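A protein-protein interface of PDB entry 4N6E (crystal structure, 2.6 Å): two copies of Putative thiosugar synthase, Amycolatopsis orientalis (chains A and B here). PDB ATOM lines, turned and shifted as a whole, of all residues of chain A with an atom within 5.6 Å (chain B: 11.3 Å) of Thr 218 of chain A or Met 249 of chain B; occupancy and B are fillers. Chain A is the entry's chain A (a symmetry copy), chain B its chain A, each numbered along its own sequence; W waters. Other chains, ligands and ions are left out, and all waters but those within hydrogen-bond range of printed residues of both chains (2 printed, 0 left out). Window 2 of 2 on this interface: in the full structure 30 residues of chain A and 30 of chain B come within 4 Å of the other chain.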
ATOM      1  N   GLN A  32      -6.484  17.810   7.789  1.00  0.00           N
ATOM      2  CA  GLN A  32      -7.080  16.477   7.646  1.00  0.00           C
ATOM      3  C   GLN A  32      -6.415  15.353   8.443  1.00  0.00           C
ATOM      4  O   GLN A  32      -7.019  14.307   8.636  1.00  0.00           O
ATOM      5  CB  GLN A  32      -7.108  16.055   6.179  1.00  0.00           C
ATOM      6  CG  GLN A  32      -7.755  17.081   5.257  1.00  0.00           C
ATOM      7  CD  GLN A  32      -7.973  16.538   3.863  1.00  0.00           C
ATOM      8  OE1 GLN A  32      -8.396  15.399   3.690  1.00  0.00           O
ATOM      9  NE2 GLN A  32      -7.678  17.346   2.862  1.00  0.00           N
ATOM     10  N   VAL A 168     -11.054  21.159  -5.389  1.00  0.00           N
ATOM     11  CA  VAL A 168     -10.422  20.675  -4.175  1.00  0.00           C
ATOM     12  C   VAL A 168     -10.659  19.183  -4.033  1.00  0.00           C
ATOM     13  O   VAL A 168     -11.771  18.732  -4.187  1.00  0.00           O
ATOM     14  CB  VAL A 168     -10.986  21.397  -2.935  1.00  0.00           C
ATOM     15  CG1 VAL A 168     -10.504  20.758  -1.634  1.00  0.00           C
ATOM     16  CG2 VAL A 168     -10.604  22.865  -2.969  1.00  0.00           C
ATOM     17  N   ALA A 169      -9.593  18.445  -3.722  1.00  0.00           N
ATOM     18  CA  ALA A 169      -9.608  16.982  -3.537  1.00  0.00           C
ATOM     19  C   ALA A 169      -9.968  16.177  -4.796  1.00  0.00           C
ATOM     20  O   ALA A 169     -10.261  14.979  -4.710  1.00  0.00           O
ATOM     21  CB  ALA A 169     -10.489  16.586  -2.350  1.00  0.00           C
ATOM     22  N   SER A 170      -9.890  16.812  -5.961  1.00  0.00           N
ATOM     23  CA  SER A 170     -10.256  16.149  -7.215  1.00  0.00           C
ATOM     24  C   SER A 170      -9.118  15.314  -7.784  1.00  0.00           C
ATOM     25  O   SER A 170      -9.362  14.385  -8.539  1.00  0.00           O
ATOM     26  CB  SER A 170     -10.702  17.163  -8.252  1.00  0.00           C
ATOM     27  OG  SER A 170      -9.603  17.936  -8.708  1.00  0.00           O
ATOM     28  N   GLY A 171      -7.879  15.644  -7.434  1.00  0.00           N
ATOM     29  CA  GLY A 171      -6.721  14.974  -8.011  1.00  0.00           C
ATOM     30  C   GLY A 171      -6.576  15.114  -9.518  1.00  0.00           C
ATOM     31  O   GLY A 171      -5.844  14.332 -10.137  1.00  0.00           O
ATOM     32  N   ILE A 197      -4.313  19.179  -6.860  1.00  0.00           N
ATOM     33  CA  ILE A 197      -3.013  18.602  -7.163  1.00  0.00           C
ATOM     34  C   ILE A 197      -3.010  17.172  -6.636  1.00  0.00           C
ATOM     35  O   ILE A 197      -3.197  16.938  -5.448  1.00  0.00           O
ATOM     36  CB  ILE A 197      -1.863  19.390  -6.531  1.00  0.00           C
ATOM     37  CG1 ILE A 197      -1.833  20.839  -7.036  1.00  0.00           C
ATOM     38  CG2 ILE A 197      -0.544  18.717  -6.847  1.00  0.00           C
ATOM     39  CD1 ILE A 197      -1.199  21.022  -8.395  1.00  0.00           C
ATOM     40  N   GLY A 198      -2.807  16.228  -7.543  1.00  0.00           N
ATOM     41  CA  GLY A 198      -2.900  14.797  -7.266  1.00  0.00           C
ATOM     42  C   GLY A 198      -1.578  14.065  -7.124  1.00  0.00           C
ATOM     43  O   GLY A 198      -1.502  13.093  -6.378  1.00  0.00           O
ATOM     44  N   VAL A 216      -0.165  21.706  -1.613  1.00  0.00           N
ATOM     45  CA  VAL A 216      -0.754  20.402  -1.736  1.00  0.00           C
ATOM     46  C   VAL A 216      -1.420  20.091  -0.423  1.00  0.00           C
ATOM     47  O   VAL A 216      -1.062  20.635   0.613  1.00  0.00           O
ATOM     48  CB  VAL A 216       0.305  19.337  -2.101  1.00  0.00           C
ATOM     49  CG1 VAL A 216       1.155  19.824  -3.273  1.00  0.00           C
ATOM     50  CG2 VAL A 216       1.211  19.018  -0.918  1.00  0.00           C
ATOM     51  N   ASN A 217      -2.396  19.207  -0.456  1.00  0.00           N
ATOM     52  CA  ASN A 217      -3.095  18.823   0.765  1.00  0.00           C
ATOM     53  C   ASN A 217      -3.601  17.388   0.682  1.00  0.00           C
ATOM     54  O   ASN A 217      -3.068  16.491   1.307  1.00  0.00           O
ATOM     55  CB  ASN A 217      -4.255  19.781   1.002  1.00  0.00           C
ATOM     56  CG  ASN A 217      -4.764  19.712   2.401  1.00  0.00           C
ATOM     57  OD1 ASN A 217      -4.761  18.656   3.005  1.00  0.00           O
ATOM     58  ND2 ASN A 217      -5.176  20.849   2.943  1.00  0.00           N
ATOM     59  N   THR A 218      -4.607  17.181  -0.142  1.00  0.00           N
ATOM     60  CA  THR A 218      -5.304  15.918  -0.201  1.00  0.00           C
ATOM     61  C   THR A 218      -4.394  14.827  -0.755  1.00  0.00           C
ATOM     62  O   THR A 218      -4.432  13.673  -0.294  1.00  0.00           O
ATOM     63  CB  THR A 218      -6.529  16.082  -1.087  1.00  0.00           C
ATOM     64  OG1 THR A 218      -7.399  17.054  -0.492  1.00  0.00           O
ATOM     65  CG2 THR A 218      -7.248  14.790  -1.245  1.00  0.00           C
ATOM     66  N   ALA A 219      -3.583  15.213  -1.735  1.00  0.00           N
ATOM     67  CA  ALA A 219      -2.604  14.319  -2.352  1.00  0.00           C
ATOM     68  C   ALA A 219      -1.715  13.574  -1.351  1.00  0.00           C
ATOM     69  O   ALA A 219      -1.415  12.413  -1.565  1.00  0.00           O
ATOM     70  CB  ALA A 219      -1.733  15.086  -3.341  1.00  0.00           C
ATOM     71  N   LEU A 220      -1.293  14.235  -0.275  1.00  0.00           N
ATOM     72  CA  LEU A 220      -0.472  13.579   0.750  1.00  0.00           C
ATOM     73  C   LEU A 220      -1.342  12.754   1.696  1.00  0.00           C
ATOM     74  O   LEU A 220      -0.975  11.648   2.105  1.00  0.00           O
ATOM     75  CB  LEU A 220       0.324  14.614   1.533  1.00  0.00           C
ATOM     76  CG  LEU A 220       1.162  15.576   0.681  1.00  0.00           C
ATOM     77  CD1 LEU A 220       1.970  16.501   1.566  1.00  0.00           C
ATOM     78  CD2 LEU A 220       2.096  14.831  -0.264  1.00  0.00           C
ATOM     79  N   VAL A 221      -2.515  13.276   2.020  1.00  0.00           N
ATOM     80  CA  VAL A 221      -3.413  12.587   2.932  1.00  0.00           C
ATOM     81  C   VAL A 221      -3.855  11.244   2.339  1.00  0.00           C
ATOM     82  O   VAL A 221      -4.055  10.277   3.069  1.00  0.00           O
ATOM     83  CB  VAL A 221      -4.649  13.452   3.263  1.00  0.00           C
ATOM     84  CG1 VAL A 221      -5.581  12.746   4.250  1.00  0.00           C
ATOM     85  CG2 VAL A 221      -4.215  14.790   3.834  1.00  0.00           C
ATOM     86  N   ARG A 222      -3.983  11.187   1.019  1.00  0.00           N
ATOM     87  CA  ARG A 222      -4.586  10.034   0.357  1.00  0.00           C
ATOM     88  C   ARG A 222      -3.644   9.213  -0.515  1.00  0.00           C
ATOM     89  O   ARG A 222      -4.092   8.329  -1.209  1.00  0.00           O
ATOM     90  CB  ARG A 222      -5.812  10.478  -0.456  1.00  0.00           C
ATOM     91  CG  ARG A 222      -6.936  10.941   0.437  1.00  0.00           C
ATOM     92  CD  ARG A 222      -8.243  11.161  -0.296  1.00  0.00           C
ATOM     93  NE  ARG A 222      -9.353  10.909   0.624  1.00  0.00           N
ATOM     94  CZ  ARG A 222     -10.035   9.763   0.722  1.00  0.00           C
ATOM     95  NH1 ARG A 222      -9.779   8.724  -0.076  1.00  0.00           N
ATOM     96  NH2 ARG A 222     -11.008   9.662   1.623  1.00  0.00           N
ATOM     97  N   ALA A 223      -2.348   9.493  -0.486  1.00  0.00           N
ATOM     98  CA  ALA A 223      -1.373   8.593  -1.106  1.00  0.00           C
ATOM     99  C   ALA A 223      -1.262   7.377  -0.204  1.00  0.00           C
ATOM    100  O   ALA A 223      -1.399   7.517   1.000  1.00  0.00           O
ATOM    101  CB  ALA A 223      -0.016   9.268  -1.251  1.00  0.00           C
ATOM    102  N   MET A 229       5.137  10.383  -1.003  1.00  0.00           N
ATOM    103  CA  MET A 229       4.598  11.405  -1.892  1.00  0.00           C
ATOM    104  C   MET A 229       5.099  12.789  -1.485  1.00  0.00           C
ATOM    105  O   MET A 229       5.411  13.604  -2.344  1.00  0.00           O
ATOM    106  CB  MET A 229       3.073  11.371  -1.970  1.00  0.00           C
ATOM    107  CG  MET A 229       2.481  12.415  -2.924  1.00  0.00           C
ATOM    108  SD  MET A 229       2.962  12.276  -4.660  1.00  0.00           S
ATOM    109  CE  MET A 229       1.856  10.960  -5.157  1.00  0.00           C
ATOM    110  N   ARG B 181       0.443   2.619 -19.838  1.00  0.00           N
ATOM    111  CA  ARG B 181       0.187   2.034 -18.520  1.00  0.00           C
ATOM    112  C   ARG B 181      -0.132   0.540 -18.653  1.00  0.00           C
ATOM    113  O   ARG B 181       0.527  -0.289 -18.033  1.00  0.00           O
ATOM    114  CB  ARG B 181      -0.966   2.742 -17.809  1.00  0.00           C
ATOM    115  CG  ARG B 181      -1.028   2.443 -16.311  1.00  0.00           C
ATOM    116  CD  ARG B 181      -2.307   2.951 -15.658  1.00  0.00           C
ATOM    117  NE  ARG B 181      -2.685   4.284 -16.135  1.00  0.00           N
ATOM    118  CZ  ARG B 181      -2.207   5.431 -15.657  1.00  0.00           C
ATOM    119  NH1 ARG B 181      -1.322   5.450 -14.651  1.00  0.00           N
ATOM    120  NH2 ARG B 181      -2.622   6.578 -16.189  1.00  0.00           N
ATOM    121  N   GLU B 208       5.264   7.877 -13.447  1.00  0.00           N
ATOM    122  CA  GLU B 208       3.991   7.608 -12.796  1.00  0.00           C
ATOM    123  C   GLU B 208       3.107   6.625 -13.557  1.00  0.00           C
ATOM    124  O   GLU B 208       2.144   6.111 -12.980  1.00  0.00           O
ATOM    125  CB  GLU B 208       3.253   8.904 -12.537  1.00  0.00           C
ATOM    126  CG  GLU B 208       3.903   9.742 -11.454  1.00  0.00           C
ATOM    127  CD  GLU B 208       3.051  10.942 -11.111  1.00  0.00           C
ATOM    128  OE1 GLU B 208       3.539  11.843 -10.388  1.00  0.00           O
ATOM    129  OE2 GLU B 208       1.885  10.969 -11.575  1.00  0.00           O
ATOM    130  N   LEU B 242       9.546   8.017  -7.020  1.00  0.00           N
ATOM    131  CA  LEU B 242       8.986   8.134  -5.680  1.00  0.00           C
ATOM    132  C   LEU B 242       7.463   8.287  -5.703  1.00  0.00           C
ATOM    133  O   LEU B 242       6.739   7.638  -4.923  1.00  0.00           O
ATOM    134  CB  LEU B 242       9.584   9.343  -4.992  1.00  0.00           C
ATOM    135  CG  LEU B 242      10.781   9.088  -4.105  1.00  0.00           C
ATOM    136  CD1 LEU B 242      11.610  10.363  -3.973  1.00  0.00           C
ATOM    137  CD2 LEU B 242      10.261   8.631  -2.752  1.00  0.00           C
ATOM    138  N   SER B 243       6.990   9.158  -6.600  1.00  0.00           N
ATOM    139  CA  SER B 243       5.566   9.435  -6.716  1.00  0.00           C
ATOM    140  C   SER B 243       4.842   8.141  -7.015  1.00  0.00           C
ATOM    141  O   SER B 243       3.894   7.763  -6.317  1.00  0.00           O
ATOM    142  CB  SER B 243       5.322  10.450  -7.819  1.00  0.00           C
ATOM    143  OG  SER B 243       3.964  10.844  -7.857  1.00  0.00           O
ATOM    144  N   TYR B 244       5.316   7.438  -8.037  1.00  0.00           N
ATOM    145  CA  TYR B 244       4.742   6.170  -8.408  1.00  0.00           C
ATOM    146  C   TYR B 244       4.661   5.187  -7.241  1.00  0.00           C
ATOM    147  O   TYR B 244       3.648   4.526  -7.049  1.00  0.00           O
ATOM    148  CB  TYR B 244       5.556   5.559  -9.522  1.00  0.00           C
ATOM    149  CG  TYR B 244       5.016   4.250 -10.003  1.00  0.00           C
ATOM    150  CD1 TYR B 244       3.891   4.193 -10.825  1.00  0.00           C
ATOM    151  CD2 TYR B 244       5.623   3.056  -9.630  1.00  0.00           C
ATOM    152  CE1 TYR B 244       3.385   2.970 -11.266  1.00  0.00           C
ATOM    153  CE2 TYR B 244       5.139   1.836 -10.067  1.00  0.00           C
ATOM    154  CZ  TYR B 244       4.027   1.792 -10.883  1.00  0.00           C
ATOM    155  OH  TYR B 244       3.577   0.564 -11.294  1.00  0.00           O
ATOM    156  N   GLU B 245       5.735   5.085  -6.471  1.00  0.00           N
ATOM    157  CA  GLU B 245       5.821   4.096  -5.411  1.00  0.00           C
ATOM    158  C   GLU B 245       4.936   4.448  -4.226  1.00  0.00           C
ATOM    159  O   GLU B 245       4.442   3.571  -3.518  1.00  0.00           O
ATOM    160  CB  GLU B 245       7.277   3.919  -5.003  1.00  0.00           C
ATOM    161  CG  GLU B 245       8.065   3.166  -6.064  1.00  0.00           C
ATOM    162  CD  GLU B 245       9.546   2.992  -5.737  1.00  0.00           C
ATOM    163  OE1 GLU B 245      10.100   3.783  -4.927  1.00  0.00           O
ATOM    164  OE2 GLU B 245      10.157   2.061  -6.329  1.00  0.00           O
ATOM    165  N   SER B 246       4.691   5.740  -4.047  1.00  0.00           N
ATOM    166  CA  SER B 246       3.843   6.235  -2.978  1.00  0.00           C
ATOM    167  C   SER B 246       2.357   5.944  -3.184  1.00  0.00           C
ATOM    168  O   SER B 246       1.549   6.263  -2.318  1.00  0.00           O
ATOM    169  CB  SER B 246       4.023   7.736  -2.842  1.00  0.00           C
ATOM    170  OG  SER B 246       3.332   8.407  -3.884  1.00  0.00           O
ATOM    171  N   GLY B 247       1.993   5.359  -4.320  1.00  0.00           N
ATOM    172  CA  GLY B 247       0.593   5.033  -4.613  1.00  0.00           C
ATOM    173  C   GLY B 247      -0.302   6.262  -4.683  1.00  0.00           C
ATOM    174  O   GLY B 247      -1.111   6.478  -3.793  1.00  0.00           O
ATOM    175  N   PRO B 248      -0.171   7.078  -5.749  1.00  0.00           N
ATOM    176  CA  PRO B 248      -0.881   8.358  -5.733  1.00  0.00           C
ATOM    177  C   PRO B 248      -2.394   8.167  -5.695  1.00  0.00           C
ATOM    178  O   PRO B 248      -2.884   7.083  -5.982  1.00  0.00           O
ATOM    179  CB  PRO B 248      -0.439   9.042  -7.040  1.00  0.00           C
ATOM    180  CG  PRO B 248       0.753   8.264  -7.517  1.00  0.00           C
ATOM    181  CD  PRO B 248       0.543   6.866  -7.024  1.00  0.00           C
ATOM    182  N   MET B 249      -3.106   9.213  -5.307  1.00  0.00           N
ATOM    183  CA  MET B 249      -4.556   9.173  -5.224  1.00  0.00           C
ATOM    184  C   MET B 249      -5.163   8.976  -6.608  1.00  0.00           C
ATOM    185  O   MET B 249      -4.683   9.554  -7.585  1.00  0.00           O
ATOM    186  CB  MET B 249      -5.087  10.477  -4.616  1.00  0.00           C
ATOM    187  CG  MET B 249      -4.857  11.720  -5.477  1.00  0.00           C
ATOM    188  SD  MET B 249      -5.399  13.259  -4.707  1.00  0.00           S
ATOM    189  CE  MET B 249      -7.181  13.011  -4.648  1.00  0.00           C
ATOM    190  N   PRO B 250      -6.211   8.148  -6.705  1.00  0.00           N
ATOM    191  CA  PRO B 250      -6.914   8.130  -7.988  1.00  0.00           C
ATOM    192  C   PRO B 250      -7.604   9.465  -8.220  1.00  0.00           C
ATOM    193  O   PRO B 250      -8.161  10.052  -7.274  1.00  0.00           O
ATOM    194  CB  PRO B 250      -7.948   7.004  -7.830  1.00  0.00           C
ATOM    195  CG  PRO B 250      -8.103   6.818  -6.358  1.00  0.00           C
ATOM    196  CD  PRO B 250      -6.797   7.220  -5.723  1.00  0.00           C
ATOM    197  N   GLU B 251      -7.523   9.943  -9.460  1.00  0.00           N
ATOM    198  CA  GLU B 251      -8.258  11.118  -9.920  1.00  0.00           C
ATOM    199  C   GLU B 251      -9.756  10.885  -9.793  1.00  0.00           C
ATOM    200  O   GLU B 251     -10.245   9.840 -10.194  1.00  0.00           O
ATOM    201  CB  GLU B 251      -7.917  11.358 -11.389  1.00  0.00           C
ATOM    202  CG  GLU B 251      -8.628  12.525 -12.050  1.00  0.00           C
ATOM    203  CD  GLU B 251      -8.408  12.554 -13.548  1.00  0.00           C
ATOM    204  OE1 GLU B 251      -7.856  11.565 -14.073  1.00  0.00           O
ATOM    205  OE2 GLU B 251      -8.797  13.556 -14.195  1.00  0.00           O
ATOM    206  N   VAL B 252     -10.478  11.855  -9.238  1.00  0.00           N
ATOM    207  CA  VAL B 252     -11.945  11.815  -9.187  1.00  0.00           C
ATOM    208  C   VAL B 252     -12.531  12.576 -10.380  1.00  0.00           C
ATOM    209  O   VAL B 252     -12.574  13.808 -10.383  1.00  0.00           O
ATOM    210  CB  VAL B 252     -12.486  12.420  -7.864  1.00  0.00           C
ATOM    211  CG1 VAL B 252     -14.013  12.447  -7.849  1.00  0.00           C
ATOM    212  CG2 VAL B 252     -11.948  11.652  -6.657  1.00  0.00           C
ATOM    213  N   ALA B 253     -12.980  11.832 -11.387  1.00  0.00           N
ATOM    214  CA  ALA B 253     -13.573  12.406 -12.605  1.00  0.00           C
ATOM    215  C   ALA B 253     -15.086  12.160 -12.648  1.00  0.00           C
ATOM    216  O   ALA B 253     -15.680  11.719 -11.660  1.00  0.00           O
ATOM    217  CB  ALA B 253     -12.900  11.811 -13.837  1.00  0.00           C
HETATM  218  O   HOH W   1      -1.836  11.136  -3.944  1.00  0.00           O
HETATM  219  O   HOH W   2      -4.168  12.054  -9.117  1.00  0.00           O
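Of the 14 printed residues of chain B, 7 touch a printed residue of chain A. Hydrophobic or aromatic side chains of chain B within 4 Å of the printed part of chain A: Pro 248, Met 249 and Val 252.
OG of Ser 243 of chain B is in hydrogen-bond range of OE1 of Glu 208 of chain B, at 2.8 Å. O of Ser 243 of chain B sits at hydrogen-bond distance from OG of Ser 246 of chain B (2.6 Å). The side-chain hydroxyl (OG1) of Thr 218 of chain A sits at hydrogen-bond distance from the side-chain amide nitrogen (NE2) of Gln 32 of chain A.
SD of Met 229 of chain A sits close to OG of Ser 243 of chain B (3.6 Å). The backbone carbonyl oxygen (O) of Ser 170 of chain A sits at hydrogen-bond distance from the backbone NH (N) of Val 252 of chain B.
No position is printed for both chains. Of the 13 pairs that touch across the chains among the printed residues, none has its exchanged pair printed and touching as well.
Of chain B, only Met 249 comes within 4 Å of Thr 218 of chain A. Of chain A, only Ala 169, Gly 171, Gly 198, Thr 218 and Ala 219 come within 4 Å of Met 249 of chain B. Ala 169 of chain A touches one residue of chain B. Ser 170 of chain A touches two residues of chain B. Of chain B, only Met 249 and Glu 251 come within 4 Å of Gly 171 of chain A. No residue of chain B comes within 4 Å of Val 216 of chain A. No residue of chain B comes within 4 Å of Asn 217 of chain A. Ala 219 of chain A touches just one residue of chain B: Met 249. No residue of chain B comes within 4 Å of Leu 220 of chain A. No residue of chain B comes within 4 Å of Val 221 of chain A. No residue of chain B comes within 4 Å of Arg 222 of chain A. Ala 223 of chain A touches two residues of chain B. Of the printed residues of chain A, Ser 243 of chain B touches Met 229 (3.4 Å). Of the printed residues of chain A, Gly 247 of chain B touches Ala 223 (3.4 Å). Of the printed residues of chain B, Met 229 of chain A touches Ser 243, Ser 246 and Pro 248. Arg 181 of chain B touches none of the printed residues of chain A. Ile 197 of chain A touches none of the printed residues of chain B. The nearest residue of chain B that does not touch Thr 218 of chain A is Pro 250 of chain B (7.7 Å). The nearest printed residue of chain A that does not touch Ser 246 of chain B is Arg 222 of chain A (6.1 Å).
Met 249 of chain B touches Ala 169 of chain A (CE to O, 3.7 Å). Met 249 of chain B touches Gly 171 of chain A. Gly 171 of chain A touches Glu 251 of chain B (O to CG, 3.8 Å). CG of Met 249 of chain B touches O of Gly 198 of chain A, 3.7 Å away. Met 249 of chain B touches Thr 218 of chain A (CE to CG2, 3.8 Å). Ala 219 of chain A touches Met 249 of chain B. O of Ser 246 of chain B touches CB of Ala 223 of chain A, 3.6 Å away. Ala 223 of chain A touches Gly 247 of chain B. OG of Ser 246 of chain B touches CE of Met 229 of chain A, at 3.2 Å. Pro 248 of chain B touches Met 229 of chain A.
Water W1 lies within hydrogen-bond range of the backbone NH (N) of Met 249 of chain B, the backbone carbonyl oxygen (O) of Ala 219 of chain A and the backbone carbonyl oxygen (O) of Gly 198 of chain A. Water W2 lies within hydrogen-bond range of the backbone carbonyl oxygen (O) of Met 249 of chain B (3.0 Å) and the backbone carbonyl oxygen (O) of Gly 171 of chain A (3.0 Å).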
